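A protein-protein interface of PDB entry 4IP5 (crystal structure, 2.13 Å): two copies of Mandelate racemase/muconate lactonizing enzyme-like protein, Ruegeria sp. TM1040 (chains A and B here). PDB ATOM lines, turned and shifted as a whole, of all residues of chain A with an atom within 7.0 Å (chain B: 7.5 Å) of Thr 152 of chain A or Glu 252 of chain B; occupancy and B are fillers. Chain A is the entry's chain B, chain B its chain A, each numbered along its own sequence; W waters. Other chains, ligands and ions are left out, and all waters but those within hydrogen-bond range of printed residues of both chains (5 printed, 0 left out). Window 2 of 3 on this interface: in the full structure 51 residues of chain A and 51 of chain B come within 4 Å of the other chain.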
ATOM      1  N   ARG A  89     -31.616 -12.390  -1.393  1.00  0.00           N
ATOM      2  CA  ARG A  89     -31.192 -12.742  -2.749  1.00  0.00           C
ATOM      3  C   ARG A  89     -31.411 -11.540  -3.664  1.00  0.00           C
ATOM      4  O   ARG A  89     -30.575 -11.232  -4.506  1.00  0.00           O
ATOM      5  CB  ARG A  89     -31.966 -13.955  -3.281  1.00  0.00           C
ATOM      6  CG  ARG A  89     -31.706 -14.285  -4.774  1.00  0.00           C
ATOM      7  CD  ARG A  89     -30.318 -14.905  -4.996  1.00  0.00           C
ATOM      8  NE  ARG A  89     -30.170 -16.106  -4.184  1.00  0.00           N
ATOM      9  CZ  ARG A  89     -30.604 -17.312  -4.547  1.00  0.00           C
ATOM     10  NH1 ARG A  89     -31.183 -17.487  -5.726  1.00  0.00           N
ATOM     11  NH2 ARG A  89     -30.459 -18.344  -3.728  1.00  0.00           N
ATOM     12  N   PHE A 148     -29.413 -19.651   1.226  1.00  0.00           N
ATOM     13  CA  PHE A 148     -28.454 -20.740   1.313  1.00  0.00           C
ATOM     14  C   PHE A 148     -27.574 -20.918   0.077  1.00  0.00           C
ATOM     15  O   PHE A 148     -26.819 -21.893   0.006  1.00  0.00           O
ATOM     16  CB  PHE A 148     -29.172 -22.062   1.611  1.00  0.00           C
ATOM     17  CG  PHE A 148     -29.513 -22.253   3.066  1.00  0.00           C
ATOM     18  CD1 PHE A 148     -28.633 -22.898   3.919  1.00  0.00           C
ATOM     19  CD2 PHE A 148     -30.714 -21.783   3.578  1.00  0.00           C
ATOM     20  CE1 PHE A 148     -28.947 -23.076   5.267  1.00  0.00           C
ATOM     21  CE2 PHE A 148     -31.040 -21.956   4.919  1.00  0.00           C
ATOM     22  CZ  PHE A 148     -30.154 -22.603   5.763  1.00  0.00           C
ATOM     23  N   ARG A 149     -27.656 -20.005  -0.891  1.00  0.00           N
ATOM     24  CA  ARG A 149     -26.874 -20.195  -2.117  1.00  0.00           C
ATOM     25  C   ARG A 149     -25.375 -20.258  -1.801  1.00  0.00           C
ATOM     26  O   ARG A 149     -24.854 -19.429  -1.055  1.00  0.00           O
ATOM     27  CB  ARG A 149     -27.175 -19.147  -3.199  1.00  0.00           C
ATOM     28  CG  ARG A 149     -26.384 -19.437  -4.504  1.00  0.00           C
ATOM     29  CD  ARG A 149     -26.866 -18.643  -5.717  1.00  0.00           C
ATOM     30  NE  ARG A 149     -26.892 -17.208  -5.454  1.00  0.00           N
ATOM     31  CZ  ARG A 149     -27.087 -16.282  -6.390  1.00  0.00           C
ATOM     32  NH1 ARG A 149     -27.254 -16.645  -7.662  1.00  0.00           N
ATOM     33  NH2 ARG A 149     -27.100 -14.993  -6.056  1.00  0.00           N
ATOM     34  N   TYR A 150     -24.727 -21.285  -2.340  1.00  0.00           N
ATOM     35  CA  TYR A 150     -23.305 -21.559  -2.144  1.00  0.00           C
ATOM     36  C   TYR A 150     -22.972 -22.092  -0.754  1.00  0.00           C
ATOM     37  O   TYR A 150     -21.805 -22.121  -0.363  1.00  0.00           O
ATOM     38  CB  TYR A 150     -22.433 -20.339  -2.474  1.00  0.00           C
ATOM     39  CG  TYR A 150     -22.674 -19.757  -3.848  1.00  0.00           C
ATOM     40  CD1 TYR A 150     -22.794 -20.580  -4.973  1.00  0.00           C
ATOM     41  CD2 TYR A 150     -22.778 -18.383  -4.026  1.00  0.00           C
ATOM     42  CE1 TYR A 150     -23.007 -20.037  -6.244  1.00  0.00           C
ATOM     43  CE2 TYR A 150     -22.991 -17.830  -5.287  1.00  0.00           C
ATOM     44  CZ  TYR A 150     -23.105 -18.655  -6.390  1.00  0.00           C
ATOM     45  OH  TYR A 150     -23.311 -18.087  -7.637  1.00  0.00           O
ATOM     46  N   LEU A 151     -23.995 -22.528  -0.021  1.00  0.00           N
ATOM     47  CA  LEU A 151     -23.791 -23.165   1.278  1.00  0.00           C
ATOM     48  C   LEU A 151     -24.116 -24.649   1.269  1.00  0.00           C
ATOM     49  O   LEU A 151     -23.684 -25.385   2.160  1.00  0.00           O
ATOM     50  CB  LEU A 151     -24.664 -22.500   2.345  1.00  0.00           C
ATOM     51  CG  LEU A 151     -24.084 -21.274   3.038  1.00  0.00           C
ATOM     52  CD1 LEU A 151     -25.044 -20.781   4.106  1.00  0.00           C
ATOM     53  CD2 LEU A 151     -22.710 -21.597   3.637  1.00  0.00           C
ATOM     54  N   THR A 152     -24.882 -25.092   0.274  1.00  0.00           N
ATOM     55  CA  THR A 152     -25.571 -26.380   0.388  1.00  0.00           C
ATOM     56  C   THR A 152     -24.670 -27.600   0.431  1.00  0.00           C
ATOM     57  O   THR A 152     -25.115 -28.665   0.849  1.00  0.00           O
ATOM     58  CB  THR A 152     -26.652 -26.584  -0.692  1.00  0.00           C
ATOM     59  OG1 THR A 152     -26.036 -26.727  -1.981  1.00  0.00           O
ATOM     60  CG2 THR A 152     -27.629 -25.414  -0.695  1.00  0.00           C
ATOM     61  N   ASP A 153     -23.412 -27.466   0.020  1.00  0.00           N
ATOM     62  CA  ASP A 153     -22.513 -28.619   0.077  1.00  0.00           C
ATOM     63  C   ASP A 153     -22.025 -28.849   1.507  1.00  0.00           C
ATOM     64  O   ASP A 153     -21.555 -29.927   1.845  1.00  0.00           O
ATOM     65  CB  ASP A 153     -21.327 -28.477  -0.890  1.00  0.00           C
ATOM     66  CG  ASP A 153     -20.472 -27.266  -0.595  1.00  0.00           C
ATOM     67  OD1 ASP A 153     -21.010 -26.255  -0.077  1.00  0.00           O
ATOM     68  OD2 ASP A 153     -19.256 -27.321  -0.883  1.00  0.00           O
ATOM     69  N   VAL A 154     -22.142 -27.829   2.343  1.00  0.00           N
ATOM     70  CA  VAL A 154     -21.685 -27.939   3.724  1.00  0.00           C
ATOM     71  C   VAL A 154     -22.858 -27.893   4.711  1.00  0.00           C
ATOM     72  O   VAL A 154     -22.895 -28.643   5.689  1.00  0.00           O
ATOM     73  CB  VAL A 154     -20.640 -26.842   4.043  1.00  0.00           C
ATOM     74  CG1 VAL A 154     -20.373 -26.754   5.530  1.00  0.00           C
ATOM     75  CG2 VAL A 154     -19.333 -27.116   3.267  1.00  0.00           C
ATOM     76  N   LEU A 155     -23.817 -27.015   4.449  1.00  0.00           N
ATOM     77  CA  LEU A 155     -25.018 -26.947   5.266  1.00  0.00           C
ATOM     78  C   LEU A 155     -26.214 -26.650   4.387  1.00  0.00           C
ATOM     79  O   LEU A 155     -26.391 -25.520   3.926  1.00  0.00           O
ATOM     80  CB  LEU A 155     -24.894 -25.870   6.348  1.00  0.00           C
ATOM     81  CG  LEU A 155     -26.092 -25.758   7.301  1.00  0.00           C
ATOM     82  CD1 LEU A 155     -26.147 -26.946   8.269  1.00  0.00           C
ATOM     83  CD2 LEU A 155     -26.062 -24.438   8.061  1.00  0.00           C
ATOM     84  N   ALA A 156     -27.024 -27.674   4.144  1.00  0.00           N
ATOM     85  CA  ALA A 156     -28.243 -27.517   3.360  1.00  0.00           C
ATOM     86  C   ALA A 156     -29.406 -27.121   4.285  1.00  0.00           C
ATOM     87  O   ALA A 156     -29.338 -27.343   5.494  1.00  0.00           O
ATOM     88  CB  ALA A 156     -28.548 -28.812   2.594  1.00  0.00           C
ATOM     89  N   PRO A 157     -30.462 -26.512   3.723  1.00  0.00           N
ATOM     90  CA  PRO A 157     -31.604 -26.071   4.533  1.00  0.00           C
ATOM     91  C   PRO A 157     -32.111 -27.140   5.509  1.00  0.00           C
ATOM     92  O   PRO A 157     -32.426 -26.840   6.667  1.00  0.00           O
ATOM     93  CB  PRO A 157     -32.663 -25.772   3.478  1.00  0.00           C
ATOM     94  CG  PRO A 157     -31.877 -25.301   2.310  1.00  0.00           C
ATOM     95  CD  PRO A 157     -30.618 -26.131   2.306  1.00  0.00           C
ATOM     96  N   GLU A 158     -32.152 -28.382   5.040  1.00  0.00           N
ATOM     97  CA  GLU A 158     -32.702 -29.485   5.815  1.00  0.00           C
ATOM     98  C   GLU A 158     -31.911 -29.681   7.112  1.00  0.00           C
ATOM     99  O   GLU A 158     -32.482 -29.788   8.202  1.00  0.00           O
ATOM    100  CB  GLU A 158     -32.695 -30.762   4.973  1.00  0.00           C
ATOM    101  CG  GLU A 158     -33.621 -30.727   3.731  1.00  0.00           C
ATOM    102  CD  GLU A 158     -33.203 -29.711   2.644  1.00  0.00           C
ATOM    103  OE1 GLU A 158     -31.989 -29.536   2.389  1.00  0.00           O
ATOM    104  OE2 GLU A 158     -34.105 -29.081   2.045  1.00  0.00           O
ATOM    105  N   GLU A 159     -30.590 -29.706   6.993  1.00  0.00           N
ATOM    106  CA  GLU A 159     -29.746 -29.868   8.161  1.00  0.00           C
ATOM    107  C   GLU A 159     -29.788 -28.632   9.062  1.00  0.00           C
ATOM    108  O   GLU A 159     -29.726 -28.751  10.286  1.00  0.00           O
ATOM    109  CB  GLU A 159     -28.314 -30.213   7.761  1.00  0.00           C
ATOM    110  CG  GLU A 159     -27.463 -30.637   8.940  1.00  0.00           C
ATOM    111  CD  GLU A 159     -26.071 -31.092   8.539  1.00  0.00           C
ATOM    112  OE1 GLU A 159     -25.351 -31.582   9.435  1.00  0.00           O
ATOM    113  OE2 GLU A 159     -25.703 -30.965   7.340  1.00  0.00           O
ATOM    114  N   LYS A 308     -17.630 -20.861   5.526  1.00  0.00           N
ATOM    115  CA  LYS A 308     -17.953 -22.280   5.468  1.00  0.00           C
ATOM    116  C   LYS A 308     -16.702 -23.116   5.213  1.00  0.00           C
ATOM    117  O   LYS A 308     -16.609 -24.251   5.675  1.00  0.00           O
ATOM    118  CB  LYS A 308     -19.020 -22.571   4.394  1.00  0.00           C
ATOM    119  CG  LYS A 308     -18.459 -22.954   3.051  1.00  0.00           C
ATOM    120  CD  LYS A 308     -19.523 -23.341   2.029  1.00  0.00           C
ATOM    121  CE  LYS A 308     -18.843 -23.543   0.670  1.00  0.00           C
ATOM    122  NZ  LYS A 308     -19.774 -23.979  -0.404  1.00  0.00           N
ATOM    123  N   GLN B 249     -20.909 -19.219 -12.520  1.00  0.00           N
ATOM    124  CA  GLN B 249     -21.054 -19.317 -11.052  1.00  0.00           C
ATOM    125  C   GLN B 249     -22.427 -19.753 -10.540  1.00  0.00           C
ATOM    126  O   GLN B 249     -22.619 -19.833  -9.330  1.00  0.00           O
ATOM    127  CB  GLN B 249     -20.676 -17.992 -10.337  1.00  0.00           C
ATOM    128  CG  GLN B 249     -19.387 -17.319 -10.808  1.00  0.00           C
ATOM    129  CD  GLN B 249     -19.346 -15.835 -10.453  1.00  0.00           C
ATOM    130  OE1 GLN B 249     -20.313 -15.288  -9.923  1.00  0.00           O
ATOM    131  NE2 GLN B 249     -18.225 -15.176 -10.751  1.00  0.00           N
ATOM    132  N   VAL B 250     -23.380 -20.037 -11.431  1.00  0.00           N
ATOM    133  CA  VAL B 250     -24.784 -20.161 -10.997  1.00  0.00           C
ATOM    134  C   VAL B 250     -25.152 -21.388 -10.149  1.00  0.00           C
ATOM    135  O   VAL B 250     -26.188 -21.390  -9.496  1.00  0.00           O
ATOM    136  CB  VAL B 250     -25.782 -20.073 -12.182  1.00  0.00           C
ATOM    137  CG1 VAL B 250     -25.625 -18.733 -12.924  1.00  0.00           C
ATOM    138  CG2 VAL B 250     -25.596 -21.247 -13.130  1.00  0.00           C
ATOM    139  N   TRP B 251     -24.321 -22.424 -10.162  1.00  0.00           N
ATOM    140  CA  TRP B 251     -24.711 -23.711  -9.586  1.00  0.00           C
ATOM    141  C   TRP B 251     -24.171 -23.952  -8.183  1.00  0.00           C
ATOM    142  O   TRP B 251     -23.119 -23.422  -7.804  1.00  0.00           O
ATOM    143  CB  TRP B 251     -24.194 -24.858 -10.463  1.00  0.00           C
ATOM    144  CG  TRP B 251     -24.784 -24.965 -11.848  1.00  0.00           C
ATOM    145  CD1 TRP B 251     -26.081 -24.747 -12.220  1.00  0.00           C
ATOM    146  CD2 TRP B 251     -24.080 -25.344 -13.046  1.00  0.00           C
ATOM    147  NE1 TRP B 251     -26.230 -24.972 -13.584  1.00  0.00           N
ATOM    148  CE2 TRP B 251     -25.014 -25.335 -14.106  1.00  0.00           C
ATOM    149  CE3 TRP B 251     -22.751 -25.688 -13.319  1.00  0.00           C
ATOM    150  CZ2 TRP B 251     -24.655 -25.650 -15.420  1.00  0.00           C
ATOM    151  CZ3 TRP B 251     -22.399 -26.007 -14.621  1.00  0.00           C
ATOM    152  CH2 TRP B 251     -23.352 -25.989 -15.656  1.00  0.00           C
ATOM    153  N   GLU B 252     -24.896 -24.783  -7.436  1.00  0.00           N
ATOM    154  CA  GLU B 252     -24.390 -25.428  -6.232  1.00  0.00           C
ATOM    155  C   GLU B 252     -23.449 -26.527  -6.705  1.00  0.00           C
ATOM    156  O   GLU B 252     -23.473 -26.905  -7.877  1.00  0.00           O
ATOM    157  CB  GLU B 252     -25.543 -26.073  -5.435  1.00  0.00           C
ATOM    158  CG  GLU B 252     -26.552 -25.066  -4.865  1.00  0.00           C
ATOM    159  CD  GLU B 252     -25.871 -24.039  -3.964  1.00  0.00           C
ATOM    160  OE1 GLU B 252     -25.874 -22.836  -4.306  1.00  0.00           O
ATOM    161  OE2 GLU B 252     -25.309 -24.448  -2.926  1.00  0.00           O
ATOM    162  N   VAL B 253     -22.648 -27.064  -5.791  1.00  0.00           N
ATOM    163  CA  VAL B 253     -21.704 -28.130  -6.125  1.00  0.00           C
ATOM    164  C   VAL B 253     -22.387 -29.379  -6.687  1.00  0.00           C
ATOM    165  O   VAL B 253     -22.002 -29.870  -7.750  1.00  0.00           O
ATOM    166  CB  VAL B 253     -20.837 -28.498  -4.895  1.00  0.00           C
ATOM    167  CG1 VAL B 253     -20.086 -29.788  -5.121  1.00  0.00           C
ATOM    168  CG2 VAL B 253     -19.880 -27.365  -4.577  1.00  0.00           C
ATOM    169  N   ASP B 254     -23.399 -29.895  -5.987  1.00  0.00           N
ATOM    170  CA  ASP B 254     -24.069 -31.120  -6.439  1.00  0.00           C
ATOM    171  C   ASP B 254     -24.798 -30.918  -7.769  1.00  0.00           C
ATOM    172  O   ASP B 254     -24.770 -31.783  -8.651  1.00  0.00           O
ATOM    173  CB  ASP B 254     -24.984 -31.723  -5.353  1.00  0.00           C
ATOM    174  CG  ASP B 254     -26.173 -30.828  -4.985  1.00  0.00           C
ATOM    175  OD1 ASP B 254     -27.076 -31.331  -4.280  1.00  0.00           O
ATOM    176  OD2 ASP B 254     -26.227 -29.646  -5.381  1.00  0.00           O
ATOM    177  N   GLU B 255     -25.417 -29.754  -7.899  1.00  0.00           N
ATOM    178  CA  GLU B 255     -26.078 -29.319  -9.125  1.00  0.00           C
ATOM    179  C   GLU B 255     -25.106 -29.178 -10.304  1.00  0.00           C
ATOM    180  O   GLU B 255     -25.427 -29.538 -11.446  1.00  0.00           O
ATOM    181  CB  GLU B 255     -26.755 -27.976  -8.849  1.00  0.00           C
ATOM    182  CG  GLU B 255     -27.393 -27.295 -10.042  1.00  0.00           C
ATOM    183  CD  GLU B 255     -28.028 -25.961  -9.653  1.00  0.00           C
ATOM    184  OE1 GLU B 255     -27.688 -25.432  -8.561  1.00  0.00           O
ATOM    185  OE2 GLU B 255     -28.871 -25.455 -10.431  1.00  0.00           O
ATOM    186  N   ALA B 256     -23.922 -28.640 -10.040  1.00  0.00           N
ATOM    187  CA  ALA B 256     -22.923 -28.469 -11.102  1.00  0.00           C
ATOM    188  C   ALA B 256     -22.483 -29.816 -11.675  1.00  0.00           C
ATOM    189  O   ALA B 256     -22.332 -29.978 -12.889  1.00  0.00           O
ATOM    190  CB  ALA B 256     -21.720 -27.705 -10.579  1.00  0.00           C
ATOM    191  N   ILE B 257     -22.288 -30.785 -10.791  1.00  0.00           N
ATOM    192  CA  ILE B 257     -21.825 -32.097 -11.206  1.00  0.00           C
ATOM    193  C   ILE B 257     -22.853 -32.782 -12.106  1.00  0.00           C
ATOM    194  O   ILE B 257     -22.519 -33.282 -13.189  1.00  0.00           O
ATOM    195  CB  ILE B 257     -21.489 -32.977  -9.990  1.00  0.00           C
ATOM    196  CG1 ILE B 257     -20.329 -32.366  -9.195  1.00  0.00           C
ATOM    197  CG2 ILE B 257     -21.173 -34.408 -10.434  1.00  0.00           C
ATOM    198  CD1 ILE B 257     -20.050 -33.080  -7.851  1.00  0.00           C
ATOM    199  N   ASP B 258     -24.104 -32.794 -11.666  1.00  0.00           N
ATOM    200  CA  ASP B 258     -25.171 -33.395 -12.460  1.00  0.00           C
ATOM    201  C   ASP B 258     -25.371 -32.740 -13.832  1.00  0.00           C
ATOM    202  O   ASP B 258     -25.563 -33.417 -14.832  1.00  0.00           O
ATOM    203  CB  ASP B 258     -26.479 -33.361 -11.681  1.00  0.00           C
ATOM    204  CG  ASP B 258     -26.451 -34.269 -10.466  1.00  0.00           C
ATOM    205  OD1 ASP B 258     -25.518 -35.106 -10.355  1.00  0.00           O
ATOM    206  OD2 ASP B 258     -27.369 -34.156  -9.630  1.00  0.00           O
ATOM    207  N   PRO B 274     -18.036 -23.300 -12.512  1.00  0.00           N
ATOM    208  CA  PRO B 274     -19.257 -24.047 -12.192  1.00  0.00           C
ATOM    209  C   PRO B 274     -19.962 -23.524 -10.925  1.00  0.00           C
ATOM    210  O   PRO B 274     -21.143 -23.797 -10.737  1.00  0.00           O
ATOM    211  CB  PRO B 274     -18.740 -25.464 -11.943  1.00  0.00           C
ATOM    212  CG  PRO B 274     -17.312 -25.268 -11.491  1.00  0.00           C
ATOM    213  CD  PRO B 274     -16.819 -24.112 -12.329  1.00  0.00           C
ATOM    214  N   THR B 275     -19.251 -22.796 -10.069  1.00  0.00           N
ATOM    215  CA  THR B 275     -19.860 -22.285  -8.846  1.00  0.00           C
ATOM    216  C   THR B 275     -19.184 -20.977  -8.402  1.00  0.00           C
ATOM    217  O   THR B 275     -18.407 -20.390  -9.166  1.00  0.00           O
ATOM    218  CB  THR B 275     -19.874 -23.372  -7.727  1.00  0.00           C
ATOM    219  OG1 THR B 275     -20.748 -22.974  -6.655  1.00  0.00           O
ATOM    220  CG2 THR B 275     -18.471 -23.658  -7.204  1.00  0.00           C
ATOM    221  N   SER B 276     -19.505 -20.516  -7.194  1.00  0.00           N
ATOM    222  CA  SER B 276     -18.963 -19.271  -6.635  1.00  0.00           C
ATOM    223  C   SER B 276     -17.448 -19.154  -6.809  1.00  0.00           C
ATOM    224  O   SER B 276     -16.717 -20.116  -6.590  1.00  0.00           O
ATOM    225  CB  SER B 276     -19.306 -19.169  -5.147  1.00  0.00           C
ATOM    226  OG  SER B 276     -18.578 -18.118  -4.520  1.00  0.00           O
ATOM    227  N   ASP B 279     -15.272 -20.308  -3.863  1.00  0.00           N
ATOM    228  CA  ASP B 279     -15.384 -21.655  -3.307  1.00  0.00           C
ATOM    229  C   ASP B 279     -14.293 -22.573  -3.859  1.00  0.00           C
ATOM    230  O   ASP B 279     -14.497 -23.265  -4.858  1.00  0.00           O
ATOM    231  CB  ASP B 279     -16.776 -22.237  -3.571  1.00  0.00           C
ATOM    232  CG  ASP B 279     -17.108 -23.420  -2.669  1.00  0.00           C
ATOM    233  OD1 ASP B 279     -16.216 -23.930  -1.953  1.00  0.00           O
ATOM    234  OD2 ASP B 279     -18.283 -23.846  -2.677  1.00  0.00           O
ATOM    235  N   GLY B 282     -15.194 -26.196  -3.042  1.00  0.00           N
ATOM    236  CA  GLY B 282     -16.304 -26.539  -3.917  1.00  0.00           C
ATOM    237  C   GLY B 282     -15.877 -26.862  -5.341  1.00  0.00           C
ATOM    238  O   GLY B 282     -16.319 -27.854  -5.919  1.00  0.00           O
ATOM    239  N   ILE B 286     -16.314 -30.396  -7.376  1.00  0.00           N
ATOM    240  CA  ILE B 286     -16.902 -30.432  -8.715  1.00  0.00           C
ATOM    241  C   ILE B 286     -15.916 -31.081  -9.685  1.00  0.00           C
ATOM    242  O   ILE B 286     -16.289 -31.937 -10.489  1.00  0.00           O
ATOM    243  CB  ILE B 286     -17.320 -29.032  -9.205  1.00  0.00           C
ATOM    244  CG1 ILE B 286     -18.476 -28.498  -8.348  1.00  0.00           C
ATOM    245  CG2 ILE B 286     -17.760 -29.080 -10.677  1.00  0.00           C
ATOM    246  CD1 ILE B 286     -18.648 -26.988  -8.415  1.00  0.00           C
HETATM  247  O   HOH W   1     -24.074 -28.921  -3.310  1.00  0.00           O
HETATM  248  O   HOH W   2     -16.900 -25.867  -0.291  1.00  0.00           O
HETATM  249  O   HOH W   3     -27.666 -28.083  -3.500  1.00  0.00           O
HETATM  250  O   HOH W   4     -27.599 -19.180  -9.132  1.00  0.00           O
HETATM  251  O   HOH W   5     -21.398 -15.919  -7.436  1.00  0.00           O
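No position is printed for both chains.
Thr 152 of chain A touches just one residue of chain B: Glu 252 (2.6 Å). Of the printed residues of chain B, Asp 153 of chain A touches Val 253. Of the printed residues of chain B, Lys 308 of chain A touches Asp 279. Of chain A, only Arg 149 (3.4 Å), Tyr 150 (2.8 Å), Leu 151 (3.7 Å) and Thr 152 (2.6 Å) come within 4 Å of Glu 252 of chain B. Of the printed residues of chain A, Val 253 of chain B touches Asp 153. Asp 258 of chain B touches none of the printed residues of chain A. The nearest printed residue of chain A that does not touch Trp 251 of chain B is Arg 149 of chain A (6.1 Å).
N of Gly 282 of chain B is in hydrogen-bond range of OD1 of Asp 279 of chain B (2.7 Å). The side-chain amino group of Lys 308 of chain A is in salt-bridge range of the side-chain carboxylate of Asp 153 of chain A (2.6 Å). The backbone carbonyl oxygen of Trp 251 of chain B lies within hydrogen-bond range of the side-chain hydroxyl of Thr 275 of chain B, at 2.7 Å. The backbone carbonyl oxygen (O) of Tyr 150 of chain A sits at hydrogen-bond distance from the side-chain amino group (NZ) of Lys 308 of chain A, 2.8 Å away. The backbone NH (N) of Glu 252 of chain B is in hydrogen-bond range of the side-chain carboxylate (OE1) of Glu 255 of chain B (3.1 Å).
Arg 149 of chain A touches Glu 252 of chain B. Tyr 150 of chain A touches Trp 251 of chain B (CE1 to O, 3.7 Å). Thr 275 of chain B touches Tyr 150 of chain A. Ser 276 of chain B touches Tyr 150 of chain A. Glu 252 of chain B touches Leu 151 of chain A (OE2 to N, 3.7 Å). Val 253 of chain B touches Asp 153 of chain A (CG2 to OD2, 3.7 Å).
Water W3 lies within hydrogen-bond range of the side-chain hydroxyl of Thr 152 of chain A (2.6 Å) and the side-chain carboxylate of Asp 254 of chain B (2.8 Å). Water W2 lies within hydrogen-bond range of the side-chain carboxylate (OD1) of Asp 279 of chain B (2.6 Å), the side-chain carboxylate (OD2) of Asp 153 of chain A (2.8 Å), the backbone NH (N) of Gly 282 of chain B (3.3 Å) and the side-chain amino group (NZ) of Lys 308 of chain A (3.4 Å). Water W4 bridges the backbone carbonyl oxygen of Val 250 of chain B and the guanidinium group of Arg 149 of chain A. Water W5 lies within hydrogen-bond range of the side-chain amide oxygen (OE1) of Gln 249 of chain B (2.8 Å) and the side-chain hydroxyl (OH) of Tyr 150 of chain A (2.9 Å). Water W1 lies within hydrogen-bond range of the backbone NH of Asp 254 of chain B (2.9 Å), the side-chain hydroxyl of Thr 152 of chain A (3.2 Å) and the backbone NH of Val 253 of chain B (3.4 Å).
Printed residues of chain A that touch a printed residue of chain B: Arg 149, Tyr 150, Leu 151, Thr 152, Asp 153 and Lys 308. Printed residues of chain B that touch a printed residue of chain A: Gln 249, Trp 251, Glu 252, Val 253, Thr 275, Ser 276 and Asp 279. Among the printed residues, Asp or Glu carboxylates within 4 Å of a Lys or Arg side-chain nitrogen of the other chain: Lys 308 of chain A with Asp 279 of chain B (2.7 Å).
NZ of Lys 308 of chain A lies within salt-bridge range of OD2 of Asp 279 of chain B, at 2.7 Å. The side-chain carboxylate of Glu 252 of chain B sits at hydrogen-bond distance from the backbone NH of Tyr 150 of chain A, 2.8 Å away. OE2 of Glu 252 of chain B is in hydrogen-bond range of OG1 of Thr 152 of chain A (2.6 Å). OH of Tyr 150 of chain A lies within hydrogen-bond range of O of Gln 249 of chain B.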
